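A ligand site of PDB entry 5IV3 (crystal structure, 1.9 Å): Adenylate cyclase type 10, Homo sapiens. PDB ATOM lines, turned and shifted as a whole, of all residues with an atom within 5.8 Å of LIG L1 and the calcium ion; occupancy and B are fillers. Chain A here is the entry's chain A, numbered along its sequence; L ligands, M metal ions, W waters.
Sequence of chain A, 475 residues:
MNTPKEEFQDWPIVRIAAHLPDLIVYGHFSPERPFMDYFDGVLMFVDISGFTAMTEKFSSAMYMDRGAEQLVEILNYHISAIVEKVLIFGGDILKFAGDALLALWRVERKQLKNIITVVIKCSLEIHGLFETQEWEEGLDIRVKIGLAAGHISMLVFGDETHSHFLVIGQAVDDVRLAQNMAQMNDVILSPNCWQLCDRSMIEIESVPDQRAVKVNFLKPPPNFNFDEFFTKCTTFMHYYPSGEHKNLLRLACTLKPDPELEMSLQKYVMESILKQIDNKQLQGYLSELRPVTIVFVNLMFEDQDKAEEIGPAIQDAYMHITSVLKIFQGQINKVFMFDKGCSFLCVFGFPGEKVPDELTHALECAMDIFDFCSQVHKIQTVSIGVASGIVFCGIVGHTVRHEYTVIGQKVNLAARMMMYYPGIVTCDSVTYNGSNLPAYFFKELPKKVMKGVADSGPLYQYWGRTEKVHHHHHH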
ATOM      1  N   PHE A  45      -5.958 -20.897   8.747  1.00  0.00           N
ATOM      2  CA  PHE A  45      -5.745 -19.494   9.105  1.00  0.00           C
ATOM      3  C   PHE A  45      -6.040 -18.665   7.916  1.00  0.00           C
ATOM      4  O   PHE A  45      -5.391 -18.835   6.837  1.00  0.00           O
ATOM      5  CB  PHE A  45      -4.323 -19.256   9.630  1.00  0.00           C
ATOM      6  CG  PHE A  45      -4.129 -17.879  10.158  1.00  0.00           C
ATOM      7  CD1 PHE A  45      -5.040 -17.315  11.079  1.00  0.00           C
ATOM      8  CD2 PHE A  45      -3.085 -17.111   9.705  1.00  0.00           C
ATOM      9  CE1 PHE A  45      -4.876 -16.027  11.513  1.00  0.00           C
ATOM     10  CE2 PHE A  45      -2.918 -15.810  10.136  1.00  0.00           C
ATOM     11  CZ  PHE A  45      -3.786 -15.274  11.048  1.00  0.00           C
ATOM     12  N   ASP A  47      -6.459 -14.889   6.571  1.00  0.00           N
ATOM     13  CA  ASP A  47      -5.974 -13.551   6.849  1.00  0.00           C
ATOM     14  C   ASP A  47      -6.359 -12.668   5.703  1.00  0.00           C
ATOM     15  O   ASP A  47      -5.859 -12.851   4.564  1.00  0.00           O
ATOM     16  CB  ASP A  47      -4.466 -13.523   7.005  1.00  0.00           C
ATOM     17  CG  ASP A  47      -3.947 -12.138   7.358  1.00  0.00           C
ATOM     18  OD1 ASP A  47      -4.628 -11.433   8.120  1.00  0.00           O
ATOM     19  OD2 ASP A  47      -2.847 -11.747   6.913  1.00  0.00           O
ATOM     20  N   ILE A  48      -7.281 -11.752   5.948  1.00  0.00           N
ATOM     21  CA  ILE A  48      -7.616 -10.708   4.966  1.00  0.00           C
ATOM     22  C   ILE A  48      -6.492  -9.668   4.991  1.00  0.00           C
ATOM     23  O   ILE A  48      -5.998  -9.288   6.057  1.00  0.00           O
ATOM     24  CB  ILE A  48      -8.906  -9.948   5.272  1.00  0.00           C
ATOM     25  CG1 ILE A  48     -10.109 -10.889   5.490  1.00  0.00           C
ATOM     26  CG2 ILE A  48      -9.168  -8.878   4.207  1.00  0.00           C
ATOM     27  CD1 ILE A  48     -10.435 -11.822   4.371  1.00  0.00           C
ATOM     28  N   SER A  49      -6.094  -9.227   3.821  1.00  0.00           N
ATOM     29  CA  SER A  49      -5.169  -8.112   3.653  1.00  0.00           C
ATOM     30  C   SER A  49      -6.052  -6.960   3.092  1.00  0.00           C
ATOM     31  O   SER A  49      -6.837  -7.148   2.130  1.00  0.00           O
ATOM     32  CB  SER A  49      -4.062  -8.493   2.681  1.00  0.00           C
ATOM     33  OG  SER A  49      -2.775  -8.271   3.246  1.00  0.00           O
ATOM     34  N   GLY A  50      -5.988  -5.819   3.780  1.00  0.00           N
ATOM     35  CA  GLY A  50      -6.443  -4.547   3.308  1.00  0.00           C
ATOM     36  C   GLY A  50      -7.339  -3.844   4.287  1.00  0.00           C
ATOM     37  O   GLY A  50      -7.623  -2.664   4.084  1.00  0.00           O
ATOM     38  N   PHE A  51      -7.853  -4.488   5.338  1.00  0.00           N
ATOM     39  CA  PHE A  51      -8.650  -3.653   6.204  1.00  0.00           C
ATOM     40  C   PHE A  51      -7.863  -2.652   7.015  1.00  0.00           C
ATOM     41  O   PHE A  51      -8.498  -1.648   7.466  1.00  0.00           O
ATOM     42  CB  PHE A  51      -9.631  -4.387   7.064  1.00  0.00           C
ATOM     43  CG  PHE A  51     -10.910  -4.642   6.360  1.00  0.00           C
ATOM     44  CD1 PHE A  51     -11.060  -5.792   5.564  1.00  0.00           C
ATOM     45  CD2 PHE A  51     -11.960  -3.731   6.451  1.00  0.00           C
ATOM     46  CE1 PHE A  51     -12.253  -6.055   4.866  1.00  0.00           C
ATOM     47  CE2 PHE A  51     -13.162  -4.002   5.771  1.00  0.00           C
ATOM     48  CZ  PHE A  51     -13.306  -5.170   4.974  1.00  0.00           C
ATOM     49  N   THR A  52      -6.545  -2.855   7.260  1.00  0.00           N
ATOM     50  CA  THR A  52      -5.846  -1.835   8.087  1.00  0.00           C
ATOM     51  C   THR A  52      -5.740  -0.521   7.310  1.00  0.00           C
ATOM     52  O   THR A  52      -6.058   0.529   7.843  1.00  0.00           O
ATOM     53  CB  THR A  52      -4.503  -2.246   8.726  1.00  0.00           C
ATOM     54  OG1 THR A  52      -4.062  -1.187   9.587  1.00  0.00           O
ATOM     55  CG2 THR A  52      -3.438  -2.428   7.720  1.00  0.00           C
ATOM     56  N   ALA A  53      -5.396  -0.560   6.019  1.00  0.00           N
ATOM     57  CA  ALA A  53      -5.587   0.624   5.131  1.00  0.00           C
ATOM     58  C   ALA A  53      -6.996   1.213   5.101  1.00  0.00           C
ATOM     59  O   ALA A  53      -7.174   2.419   5.234  1.00  0.00           O
ATOM     60  CB  ALA A  53      -5.187   0.295   3.701  1.00  0.00           C
ATOM     61  N   ALA A  97      -8.698 -12.094  15.181  1.00  0.00           N
ATOM     62  CA  ALA A  97      -7.728 -11.031  15.455  1.00  0.00           C
ATOM     63  C   ALA A  97      -7.781 -10.084  14.304  1.00  0.00           C
ATOM     64  O   ALA A  97      -7.371 -10.406  13.159  1.00  0.00           O
ATOM     65  CB  ALA A  97      -6.355 -11.596  15.567  1.00  0.00           C
ATOM     66  N   ASP A  99      -8.681  -8.553  11.221  1.00  0.00           N
ATOM     67  CA  ASP A  99      -9.326  -9.081  10.005  1.00  0.00           C
ATOM     68  C   ASP A  99      -8.882 -10.511   9.630  1.00  0.00           C
ATOM     69  O   ASP A  99      -8.940 -10.900   8.425  1.00  0.00           O
ATOM     70  CB  ASP A  99      -9.099  -8.087   8.836  1.00  0.00           C
ATOM     71  CG  ASP A  99      -7.649  -7.860   8.527  1.00  0.00           C
ATOM     72  OD1 ASP A  99      -6.785  -8.531   9.133  1.00  0.00           O
ATOM     73  OD2 ASP A  99      -7.363  -6.924   7.782  1.00  0.00           O
ATOM     74  N   ALA A 100      -8.466 -11.290  10.640  1.00  0.00           N
ATOM     75  CA  ALA A 100      -8.038 -12.661  10.465  1.00  0.00           C
ATOM     76  C   ALA A 100      -8.767 -13.536  11.427  1.00  0.00           C
ATOM     77  O   ALA A 100      -9.216 -13.067  12.497  1.00  0.00           O
ATOM     78  CB  ALA A 100      -6.564 -12.756  10.766  1.00  0.00           C
ATOM     79  N   LYS A 144      -5.706 -14.471   2.179  1.00  0.00           N
ATOM     80  CA  LYS A 144      -4.661 -15.476   2.142  1.00  0.00           C
ATOM     81  C   LYS A 144      -5.020 -16.597   3.123  1.00  0.00           C
ATOM     82  O   LYS A 144      -5.398 -16.306   4.269  1.00  0.00           O
ATOM     83  CB  LYS A 144      -3.321 -14.874   2.533  1.00  0.00           C
ATOM     84  CG  LYS A 144      -2.851 -13.668   1.705  1.00  0.00           C
ATOM     85  CD  LYS A 144      -1.513 -13.123   2.242  1.00  0.00           C
ATOM     86  CE  LYS A 144      -1.127 -11.867   1.493  1.00  0.00           C
ATOM     87  NZ  LYS A 144       0.328 -11.589   1.679  1.00  0.00           N
ATOM     88  N   ARG A 176       0.482 -20.744  10.350  1.00  0.00           N
ATOM     89  CA  ARG A 176       0.854 -19.342  10.197  1.00  0.00           C
ATOM     90  C   ARG A 176       1.955 -19.138   9.112  1.00  0.00           C
ATOM     91  O   ARG A 176       1.842 -18.221   8.269  1.00  0.00           O
ATOM     92  CB  ARG A 176       1.285 -18.742  11.499  1.00  0.00           C
ATOM     93  CG  ARG A 176       1.002 -17.239  11.408  1.00  0.00           C
ATOM     94  CD  ARG A 176       2.087 -16.371  11.908  1.00  0.00           C
ATOM     95  NE  ARG A 176       3.430 -16.776  11.499  1.00  0.00           N
ATOM     96  CZ  ARG A 176       4.252 -16.091  10.666  1.00  0.00           C
ATOM     97  NH1 ARG A 176       5.482 -16.549  10.470  1.00  0.00           N
ATOM     98  NH2 ARG A 176       3.871 -14.969  10.037  1.00  0.00           N
ATOM     99  N   GLN A 179       0.168 -19.610   5.553  1.00  0.00           N
ATOM    100  CA  GLN A 179      -0.618 -18.464   5.164  1.00  0.00           C
ATOM    101  C   GLN A 179       0.259 -17.277   4.723  1.00  0.00           C
ATOM    102  O   GLN A 179      -0.088 -16.512   3.827  1.00  0.00           O
ATOM    103  CB  GLN A 179      -1.524 -18.005   6.359  1.00  0.00           C
ATOM    104  CG  GLN A 179      -2.149 -16.629   6.148  1.00  0.00           C
ATOM    105  CD  GLN A 179      -1.278 -15.517   6.689  1.00  0.00           C
ATOM    106  OE1 GLN A 179      -0.640 -15.666   7.707  1.00  0.00           O
ATOM    107  NE2 GLN A 179      -1.275 -14.435   6.050  1.00  0.00           N
ATOM    108  N   ASN A 180       1.347 -17.069   5.456  1.00  0.00           N
ATOM    109  CA  ASN A 180       2.261 -15.938   5.186  1.00  0.00           C
ATOM    110  C   ASN A 180       2.983 -16.000   3.796  1.00  0.00           C
ATOM    111  O   ASN A 180       3.434 -14.975   3.285  1.00  0.00           O
ATOM    112  CB  ASN A 180       3.260 -15.900   6.321  1.00  0.00           C
ATOM    113  CG  ASN A 180       4.039 -14.606   6.371  1.00  0.00           C
ATOM    114  OD1 ASN A 180       3.475 -13.540   6.272  1.00  0.00           O
ATOM    115  ND2 ASN A 180       5.337 -14.716   6.511  1.00  0.00           N
ATOM    116  N   PHE A 336      -2.017 -14.404  21.545  1.00  0.00           N
ATOM    117  CA  PHE A 336      -1.585 -15.157  20.341  1.00  0.00           C
ATOM    118  C   PHE A 336      -0.321 -15.952  20.681  1.00  0.00           C
ATOM    119  O   PHE A 336       0.456 -15.528  21.537  1.00  0.00           O
ATOM    120  CB  PHE A 336      -1.078 -14.234  19.254  1.00  0.00           C
ATOM    121  CG  PHE A 336      -1.947 -13.123  18.965  1.00  0.00           C
ATOM    122  CD1 PHE A 336      -3.039 -13.326  18.210  1.00  0.00           C
ATOM    123  CD2 PHE A 336      -1.695 -11.861  19.479  1.00  0.00           C
ATOM    124  CE1 PHE A 336      -3.896 -12.260  17.937  1.00  0.00           C
ATOM    125  CE2 PHE A 336      -2.506 -10.797  19.178  1.00  0.00           C
ATOM    126  CZ  PHE A 336      -3.617 -10.982  18.413  1.00  0.00           C
ATOM    127  N   PHE A 338       2.816 -18.188  18.260  1.00  0.00           N
ATOM    128  CA  PHE A 338       3.390 -18.924  17.081  1.00  0.00           C
ATOM    129  C   PHE A 338       4.896 -18.651  17.098  1.00  0.00           C
ATOM    130  O   PHE A 338       5.315 -17.724  17.792  1.00  0.00           O
ATOM    131  CB  PHE A 338       2.746 -18.517  15.770  1.00  0.00           C
ATOM    132  CG  PHE A 338       2.697 -17.037  15.569  1.00  0.00           C
ATOM    133  CD1 PHE A 338       3.771 -16.361  14.967  1.00  0.00           C
ATOM    134  CD2 PHE A 338       1.567 -16.309  15.949  1.00  0.00           C
ATOM    135  CE1 PHE A 338       3.709 -14.965  14.777  1.00  0.00           C
ATOM    136  CE2 PHE A 338       1.511 -14.917  15.743  1.00  0.00           C
ATOM    137  CZ  PHE A 338       2.593 -14.251  15.184  1.00  0.00           C
ATOM    138  N   ASN A 412      -0.526  -2.761  14.139  1.00  0.00           N
ATOM    139  CA  ASN A 412       0.500  -3.354  13.320  1.00  0.00           C
ATOM    140  C   ASN A 412       1.907  -2.784  13.673  1.00  0.00           C
ATOM    141  O   ASN A 412       2.882  -3.551  13.746  1.00  0.00           O
ATOM    142  CB  ASN A 412       0.247  -3.123  11.816  1.00  0.00           C
ATOM    143  CG  ASN A 412      -0.979  -3.887  11.310  1.00  0.00           C
ATOM    144  OD1 ASN A 412      -1.710  -4.431  12.112  1.00  0.00           O
ATOM    145  ND2 ASN A 412      -1.172  -3.930   9.996  1.00  0.00           N
ATOM    146  N   ARG A 416       5.151  -4.935  14.934  1.00  0.00           N
ATOM    147  CA  ARG A 416       6.418  -4.869  14.196  1.00  0.00           C
ATOM    148  C   ARG A 416       7.606  -4.415  15.056  1.00  0.00           C
ATOM    149  O   ARG A 416       8.664  -5.062  15.008  1.00  0.00           O
ATOM    150  CB  ARG A 416       6.281  -3.974  12.993  1.00  0.00           C
ATOM    151  CG  ARG A 416       5.367  -4.522  11.929  1.00  0.00           C
ATOM    152  CD  ARG A 416       6.029  -5.560  11.045  1.00  0.00           C
ATOM    153  NE  ARG A 416       5.031  -6.403  10.348  1.00  0.00           N
ATOM    154  CZ  ARG A 416       4.731  -7.685  10.631  1.00  0.00           C
ATOM    155  NH1 ARG A 416       5.348  -8.371  11.598  1.00  0.00           N
ATOM    156  NH2 ARG A 416       3.808  -8.300   9.908  1.00  0.00           N
ATOM    157  N   LYS A 451       8.732  -4.643   7.476  1.00  0.00           N
ATOM    158  CA  LYS A 451       7.875  -5.263   6.431  1.00  0.00           C
ATOM    159  C   LYS A 451       6.389  -4.984   6.693  1.00  0.00           C
ATOM    160  O   LYS A 451       5.879  -5.298   7.774  1.00  0.00           O
ATOM    161  CB  LYS A 451       8.137  -6.788   6.302  1.00  0.00           C
ATOM    162  N   GLY A 452       5.738  -4.382   5.699  1.00  0.00           N
ATOM    163  CA  GLY A 452       4.373  -3.889   5.834  1.00  0.00           C
ATOM    164  C   GLY A 452       4.213  -2.618   6.665  1.00  0.00           C
ATOM    165  O   GLY A 452       3.172  -2.424   7.287  1.00  0.00           O
HETATM  166  P1  LIG L   1      -3.821  -5.878   6.995  1.00  0.00           P
HETATM  167  O1  LIG L   1      -3.057  -5.358   8.141  1.00  0.00           O
HETATM  168  O2  LIG L   1      -4.961  -6.674   7.530  1.00  0.00           O
HETATM  169  O3  LIG L   1      -4.847  -5.034   6.220  1.00  0.00           O
HETATM  170  P2  LIG L   1      -1.949  -8.050   6.658  1.00  0.00           P
HETATM  171  O4  LIG L   1      -2.291  -9.334   7.486  1.00  0.00           O
HETATM  172  O5  LIG L   1      -1.401  -8.366   5.325  1.00  0.00           O
HETATM  173  O6  LIG L   1      -3.082  -7.001   6.133  1.00  0.00           O
HETATM  174  P3  LIG L   1       0.904  -7.867   7.515  1.00  0.00           P
HETATM  175  O7  LIG L   1       1.950  -7.053   8.430  1.00  0.00           O
HETATM  176  O8  LIG L   1       1.385  -7.802   6.087  1.00  0.00           O
HETATM  177  C1  LIG L   1      -0.773  -7.188   7.723  1.00  0.00           C
HETATM  178  O9  LIG L   1       0.866  -9.367   7.993  1.00  0.00           O
HETATM  179  C2  LIG L   1       2.119  -9.986   7.620  1.00  0.00           C
HETATM  180  C3  LIG L   1       2.197 -11.339   8.237  1.00  0.00           C
HETATM  181  O10 LIG L   1       2.220 -11.318   9.675  1.00  0.00           O
HETATM  182  C4  LIG L   1       0.895 -12.031   7.813  1.00  0.00           C
HETATM  183  O11 LIG L   1       0.965 -12.424   6.439  1.00  0.00           O
HETATM  184  C5  LIG L   1       0.724 -13.078   8.889  1.00  0.00           C
HETATM  185  O12 LIG L   1       1.509 -14.248   8.675  1.00  0.00           O
HETATM  186  C6  LIG L   1       1.232 -12.286  10.086  1.00  0.00           C
HETATM  187  N1  LIG L   1      -0.010 -11.715  10.725  1.00  0.00           N
HETATM  188  C7  LIG L   1      -0.795 -10.612  10.479  1.00  0.00           C
HETATM  189  N2  LIG L   1      -1.818 -10.580  11.368  1.00  0.00           N
HETATM  190  C8  LIG L   1      -1.695 -11.700  12.166  1.00  0.00           C
HETATM  191  C9  LIG L   1      -2.355 -12.377  13.321  1.00  0.00           C
HETATM  192  N3  LIG L   1      -3.430 -11.901  13.884  1.00  0.00           N
HETATM  193  N4  LIG L   1      -1.868 -13.498  13.860  1.00  0.00           N
HETATM  194  C10 LIG L   1      -0.748 -14.082  13.389  1.00  0.00           C
HETATM  195  N5  LIG L   1      -0.083 -13.558  12.357  1.00  0.00           N
HETATM  196  C11 LIG L   1      -0.506 -12.414  11.746  1.00  0.00           C
HETATM  197  C1  LG2 L   2      -2.477 -17.484  13.747  1.00  0.00           C
HETATM  198  C2  LG2 L   2      -2.030 -18.606  13.131  1.00  0.00           C
HETATM  199  C3  LG2 L   2      -1.523 -19.620  13.906  1.00  0.00           C
HETATM  200  S1  LG2 L   2      -1.492 -19.024  15.463  1.00  0.00           S
HETATM  201  C4  LG2 L   2      -2.203 -17.535  15.075  1.00  0.00           C
HETATM  202  C5  LG2 L   2      -2.510 -16.506  16.175  1.00  0.00           C
HETATM  203  N1  LG2 L   2      -3.810 -16.741  16.781  1.00  0.00           N
HETATM  204  C6  LG2 L   2      -4.953 -16.369  15.919  1.00  0.00           C
HETATM  205  C7  LG2 L   2      -6.051 -15.425  16.492  1.00  0.00           C
HETATM  206  C8  LG2 L   2      -4.973 -14.944  15.522  1.00  0.00           C
HETATM  207  C9  LG2 L   2      -3.912 -17.665  17.723  1.00  0.00           C
HETATM  208  N2  LG2 L   2      -2.808 -18.229  18.208  1.00  0.00           N
HETATM  209  C10 LG2 L   2      -5.141 -18.136  18.182  1.00  0.00           C
HETATM  210  C11 LG2 L   2      -5.113 -19.168  19.089  1.00  0.00           C
HETATM  211 CL1  LG2 L   2      -6.549 -19.864  19.693  1.00  0.00          CL
HETATM  212  N3  LG2 L   2      -3.987 -19.723  19.441  1.00  0.00           N
HETATM  213  C12 LG2 L   2      -2.832 -19.241  19.017  1.00  0.00           C
HETATM  214  N4  LG2 L   2      -1.694 -19.798  19.417  1.00  0.00           N
HETATM  215 CA    CA M   1      -4.730  -9.140   8.176  1.00  0.00          CA
HETATM  216  O   HOH W   1      -3.905  -2.877   5.014  1.00  0.00           O
HETATM  217  O   HOH W   2      -4.615 -10.155  12.687  1.00  0.00           O
HETATM  218  O   HOH W   3      -3.754  -8.615  10.338  1.00  0.00           O
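O12 of LIG L1 sits at hydrogen-bond distance from OE1 of Gln 179.
ND2 of Asn 412 lies within hydrogen-bond range of O1 of LIG L1, 3.0 Å away.
The backbone NH (N) of Thr 52 is in hydrogen-bond range of an oxygen (O3) of LIG L1 (3.0 Å).
The backbone NH (N) of Gly 50 is in hydrogen-bond range of an oxygen (O3) of LIG L1, at 2.8 Å.
An oxygen (O5) of LIG L1 sits at hydrogen-bond distance from the side-chain hydroxyl (OG) of Ser 49 (2.5 Å).
The side-chain amide oxygen (OD1) of Asn 180 lies within hydrogen-bond range of an oxygen (O11) of LIG L1.
NH2 of Arg 176 sits at hydrogen-bond distance from O12 of LIG L1.
NH2 of Arg 416 lies within salt-bridge range of O7 of LIG L1.
O3 of LIG L1 sits at hydrogen-bond distance from N of Phe 51.
N of Phe 51 lies close to OD2 of Asp 99.
OD2 of Asp 47 lies within hydrogen-bond range of NE2 of Gln 179 (3.2 Å).
The backbone NH (N) of Lys 144 lies within hydrogen-bond range of the backbone carbonyl oxygen (O) of Asp 47 (2.9 Å).
The guanidinium group (NE) of Arg 416 sits at hydrogen-bond distance from the backbone carbonyl oxygen (O) of Lys 451 (2.9 Å).
Merely in contact with LIG L1: Phe 338, Ala 97 and Phe 45.
Hydrophobic or aromatic side chains that line LIG L1: Phe 45, Ala 97 and Phe 338.
15 residues have an atom within 4 Å of LIG L1: Phe 45, Asp 47, Ile 48, Ser 49, Gly 50, Phe 51, Thr 52, Ala 97, Asp 99, Arg 176, Gln 179, Asn 180, Phe 338, Asn 412 and Arg 416.
The nearest printed residue that does not touch LIG L1 is Phe 336 (4.1 Å).
Within 4 Å of the calcium ion: Asp 47, Ile 48 and Asp 99.
OD1 of Asp 47 is bound to the calcium ion (2.3 Å).
The calcium ion is bound by the side-chain carboxylate (OD1) of Asp 99, at 2.3 Å.
Water W3 is bound to the calcium ion, at 2.4 Å.
The calcium ion is bound by O of Ile 48.
The calcium ion is bound by O4 of LIG L1, 2.5 Å away.
The calcium ion is bound by O2 of LIG L1 (2.6 Å).
The calcium ion has six donor atoms within binding distance.
Water W2 bridges a nitrogen (N3) of LIG L1 (2.4 Å) and the backbone carbonyl oxygen (O) of Ala 97 (2.8 Å).
Water W1 lies within hydrogen-bond range of an oxygen (O3) of LIG L1 (2.6 Å), the backbone NH of Ala 53 (2.9 Å) and the backbone NH of Thr 52 (3.5 Å).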
